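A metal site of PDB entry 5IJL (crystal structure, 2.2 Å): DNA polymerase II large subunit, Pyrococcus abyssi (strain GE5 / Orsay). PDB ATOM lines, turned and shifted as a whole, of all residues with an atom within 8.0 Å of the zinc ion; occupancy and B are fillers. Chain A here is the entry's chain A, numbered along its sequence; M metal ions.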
ATOM      1  N   LYS A 710      21.904  31.692  26.302  1.00  0.00           N
ATOM      2  CA  LYS A 710      22.422  31.050  25.101  1.00  0.00           C
ATOM      3  C   LYS A 710      23.019  29.694  25.429  1.00  0.00           C
ATOM      4  O   LYS A 710      23.809  29.576  26.364  1.00  0.00           O
ATOM      5  CB  LYS A 710      23.473  31.940  24.411  1.00  0.00           C
ATOM      6  CG  LYS A 710      23.848  31.485  23.004  1.00  0.00           C
ATOM      7  CD  LYS A 710      24.789  32.480  22.343  1.00  0.00           C
ATOM      8  CE  LYS A 710      25.177  32.076  20.948  1.00  0.00           C
ATOM      9  NZ  LYS A 710      26.192  33.002  20.391  1.00  0.00           N
ATOM     10  N   CYS A 711      22.672  28.673  24.621  1.00  0.00           N
ATOM     11  CA  CYS A 711      23.219  27.327  24.787  1.00  0.00           C
ATOM     12  C   CYS A 711      24.630  27.247  24.162  1.00  0.00           C
ATOM     13  O   CYS A 711      24.790  27.587  22.983  1.00  0.00           O
ATOM     14  CB  CYS A 711      22.292  26.273  24.205  1.00  0.00           C
ATOM     15  SG  CYS A 711      22.891  24.575  24.392  1.00  0.00           S
ATOM     16  N   PRO A 712      25.646  26.785  24.924  1.00  0.00           N
ATOM     17  CA  PRO A 712      26.989  26.634  24.333  1.00  0.00           C
ATOM     18  C   PRO A 712      27.095  25.440  23.360  1.00  0.00           C
ATOM     19  O   PRO A 712      27.932  25.466  22.457  1.00  0.00           O
ATOM     20  CB  PRO A 712      27.912  26.453  25.544  1.00  0.00           C
ATOM     21  CG  PRO A 712      27.033  26.553  26.769  1.00  0.00           C
ATOM     22  CD  PRO A 712      25.630  26.315  26.322  1.00  0.00           C
ATOM     23  N   LYS A 713      26.242  24.396  23.546  1.00  0.00           N
ATOM     24  CA  LYS A 713      26.208  23.173  22.745  1.00  0.00           C
ATOM     25  C   LYS A 713      25.653  23.410  21.321  1.00  0.00           C
ATOM     26  O   LYS A 713      26.366  23.151  20.359  1.00  0.00           O
ATOM     27  CB  LYS A 713      25.451  22.048  23.496  1.00  0.00           C
ATOM     28  CG  LYS A 713      25.543  20.642  22.869  1.00  0.00           C
ATOM     29  CD  LYS A 713      26.704  19.796  23.433  1.00  0.00           C
ATOM     30  CE  LYS A 713      26.304  18.863  24.549  1.00  0.00           C
ATOM     31  NZ  LYS A 713      27.425  17.991  24.976  1.00  0.00           N
ATOM     32  N   CYS A 714      24.399  23.892  21.197  1.00  0.00           N
ATOM     33  CA  CYS A 714      23.758  24.120  19.900  1.00  0.00           C
ATOM     34  C   CYS A 714      23.728  25.595  19.483  1.00  0.00           C
ATOM     35  O   CYS A 714      24.049  25.906  18.337  1.00  0.00           O
ATOM     36  CB  CYS A 714      22.373  23.481  19.837  1.00  0.00           C
ATOM     37  SG  CYS A 714      21.144  24.229  20.947  1.00  0.00           S
ATOM     38  N   GLY A 715      23.345  26.472  20.415  1.00  0.00           N
ATOM     39  CA  GLY A 715      23.269  27.908  20.180  1.00  0.00           C
ATOM     40  C   GLY A 715      21.915  28.532  20.433  1.00  0.00           C
ATOM     41  O   GLY A 715      21.720  29.702  20.102  1.00  0.00           O
ATOM     42  N   HIS A 716      20.985  27.761  21.042  1.00  0.00           N
ATOM     43  CA  HIS A 716      19.614  28.196  21.341  1.00  0.00           C
ATOM     44  C   HIS A 716      19.572  29.411  22.278  1.00  0.00           C
ATOM     45  O   HIS A 716      20.307  29.443  23.265  1.00  0.00           O
ATOM     46  CB  HIS A 716      18.762  27.034  21.898  1.00  0.00           C
ATOM     47  CG  HIS A 716      17.350  27.428  22.243  1.00  0.00           C
ATOM     48  ND1 HIS A 716      16.332  27.370  21.312  1.00  0.00           N
ATOM     49  CD2 HIS A 716      16.846  27.899  23.406  1.00  0.00           C
ATOM     50  CE1 HIS A 716      15.241  27.793  21.934  1.00  0.00           C
ATOM     51  NE2 HIS A 716      15.507  28.117  23.193  1.00  0.00           N
ATOM     52  N   VAL A 717      18.716  30.397  21.956  1.00  0.00           N
ATOM     53  CA  VAL A 717      18.518  31.618  22.738  1.00  0.00           C
ATOM     54  C   VAL A 717      17.047  31.713  23.202  1.00  0.00           C
ATOM     55  O   VAL A 717      16.113  31.631  22.399  1.00  0.00           O
ATOM     56  CB  VAL A 717      19.029  32.893  22.019  1.00  0.00           C
ATOM     57  CG1 VAL A 717      18.684  34.159  22.794  1.00  0.00           C
ATOM     58  CG2 VAL A 717      20.533  32.834  21.770  1.00  0.00           C
ATOM     59  N   LEU A 722      17.553  25.770  31.081  1.00  0.00           N
ATOM     60  CA  LEU A 722      17.944  24.559  30.365  1.00  0.00           C
ATOM     61  C   LEU A 722      17.541  24.650  28.913  1.00  0.00           C
ATOM     62  O   LEU A 722      16.480  25.190  28.600  1.00  0.00           O
ATOM     63  CB  LEU A 722      17.324  23.274  30.974  1.00  0.00           C
ATOM     64  CG  LEU A 722      17.873  22.703  32.277  1.00  0.00           C
ATOM     65  CD1 LEU A 722      17.209  21.374  32.561  1.00  0.00           C
ATOM     66  CD2 LEU A 722      19.378  22.523  32.230  1.00  0.00           C
ATOM     67  N   CYS A 723      18.384  24.095  28.020  1.00  0.00           N
ATOM     68  CA  CYS A 723      18.099  24.071  26.591  1.00  0.00           C
ATOM     69  C   CYS A 723      16.921  23.123  26.250  1.00  0.00           C
ATOM     70  O   CYS A 723      16.918  21.976  26.708  1.00  0.00           O
ATOM     71  CB  CYS A 723      19.352  23.734  25.789  1.00  0.00           C
ATOM     72  SG  CYS A 723      19.177  24.009  24.008  1.00  0.00           S
ATOM     73  N   PRO A 724      15.897  23.586  25.495  1.00  0.00           N
ATOM     74  CA  PRO A 724      14.787  22.691  25.151  1.00  0.00           C
ATOM     75  C   PRO A 724      15.149  21.661  24.075  1.00  0.00           C
ATOM     76  O   PRO A 724      14.382  20.713  23.834  1.00  0.00           O
ATOM     77  CB  PRO A 724      13.687  23.652  24.685  1.00  0.00           C
ATOM     78  CG  PRO A 724      14.422  24.833  24.152  1.00  0.00           C
ATOM     79  CD  PRO A 724      15.725  24.924  24.884  1.00  0.00           C
ATOM     80  N   ASN A 725      16.310  21.856  23.433  1.00  0.00           N
ATOM     81  CA  ASN A 725      16.854  21.005  22.377  1.00  0.00           C
ATOM     82  C   ASN A 725      17.757  19.906  22.905  1.00  0.00           C
ATOM     83  O   ASN A 725      17.487  18.737  22.617  1.00  0.00           O
ATOM     84  CB  ASN A 725      17.564  21.852  21.320  1.00  0.00           C
ATOM     85  CG  ASN A 725      16.616  22.629  20.448  1.00  0.00           C
ATOM     86  OD1 ASN A 725      15.999  23.607  20.860  1.00  0.00           O
ATOM     87  ND2 ASN A 725      16.469  22.190  19.212  1.00  0.00           N
ATOM     88  N   CYS A 726      18.814  20.253  23.667  1.00  0.00           N
ATOM     89  CA  CYS A 726      19.760  19.262  24.191  1.00  0.00           C
ATOM     90  C   CYS A 726      19.764  19.135  25.726  1.00  0.00           C
ATOM     91  O   CYS A 726      20.432  18.242  26.267  1.00  0.00           O
ATOM     92  CB  CYS A 726      21.167  19.499  23.638  1.00  0.00           C
ATOM     93  SG  CYS A 726      21.748  21.208  23.782  1.00  0.00           S
ATOM     94  N   GLY A 727      19.013  19.998  26.405  1.00  0.00           N
ATOM     95  CA  GLY A 727      18.868  19.988  27.858  1.00  0.00           C
ATOM     96  C   GLY A 727      20.090  20.400  28.669  1.00  0.00           C
ATOM     97  O   GLY A 727      20.121  20.153  29.868  1.00  0.00           O
ATOM     98  N   THR A 728      21.099  21.015  28.018  1.00  0.00           N
ATOM     99  CA  THR A 728      22.305  21.503  28.698  1.00  0.00           C
ATOM    100  C   THR A 728      22.040  22.901  29.279  1.00  0.00           C
ATOM    101  O   THR A 728      21.248  23.653  28.704  1.00  0.00           O
ATOM    102  CB  THR A 728      23.568  21.430  27.798  1.00  0.00           C
ATOM    103  OG1 THR A 728      23.286  21.982  26.510  1.00  0.00           O
ATOM    104  CG2 THR A 728      24.095  20.019  27.649  1.00  0.00           C
ATOM    105  N   ARG A 729      22.676  23.216  30.427  1.00  0.00           N
ATOM    106  CA  ARG A 729      22.505  24.521  31.063  1.00  0.00           C
ATOM    107  C   ARG A 729      23.057  25.667  30.206  1.00  0.00           C
ATOM    108  O   ARG A 729      24.217  25.681  29.823  1.00  0.00           O
ATOM    109  CB  ARG A 729      23.096  24.555  32.486  1.00  0.00           C
ATOM    110  CG  ARG A 729      22.743  25.835  33.266  1.00  0.00           C
ATOM    111  CD  ARG A 729      22.668  25.538  34.727  1.00  0.00           C
ATOM    112  NE  ARG A 729      22.803  26.731  35.559  1.00  0.00           N
ATOM    113  CZ  ARG A 729      21.780  27.384  36.100  1.00  0.00           C
ATOM    114  NH1 ARG A 729      20.535  26.981  35.873  1.00  0.00           N
ATOM    115  NH2 ARG A 729      21.998  28.448  36.863  1.00  0.00           N
ATOM    116  N   LYS A 730      22.186  26.628  29.941  1.00  0.00           N
ATOM    117  CA  LYS A 730      22.446  27.802  29.103  1.00  0.00           C
ATOM    118  C   LYS A 730      23.103  28.951  29.877  1.00  0.00           C
ATOM    119  O   LYS A 730      22.901  29.093  31.071  1.00  0.00           O
ATOM    120  CB  LYS A 730      21.137  28.255  28.445  1.00  0.00           C
ATOM    121  CG  LYS A 730      20.499  27.203  27.531  1.00  0.00           C
ATOM    122  CD  LYS A 730      19.014  27.484  27.367  1.00  0.00           C
ATOM    123  CE  LYS A 730      18.702  28.413  26.233  1.00  0.00           C
ATOM    124  NZ  LYS A 730      17.377  29.025  26.389  1.00  0.00           N
HETATM  125 ZN    ZN M   1      21.263  23.427  23.156  1.00  0.00          ZN
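SG of Cys 711 sits close to OG1 of Thr 728, at 3.4 Å. The backbone NH (N) of Lys 713 lies close to the side-chain sulfur (SG) of Cys 711 (3.5 Å). The side-chain sulfur (SG) of Cys 726 lies close to the side-chain hydroxyl (OG1) of Thr 728, at 3.2 Å. N of Cys 723 lies within hydrogen-bond range of O of Thr 728, at 3.0 Å. The backbone NH (N) of Cys 711 lies within hydrogen-bond range of the backbone carbonyl oxygen (O) of His 716 (2.8 Å). N of Asn 725 sits close to SG of Cys 723 (3.6 Å). SG of Cys 714 lies close to N of His 716 (3.5 Å).
The zinc ion is bound by SG of Cys 723 (2.3 Å), SG of Cys 711 (2.3 Å), SG of Cys 714 (2.4 Å) and SG of Cys 726 (2.4 Å).
Four residues have an atom within 4 Å of the zinc ion: Cys 711, Cys 714, Cys 723 and Cys 726. The nearest printed residue that does not touch the zinc ion is Thr 728 (4.2 Å).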
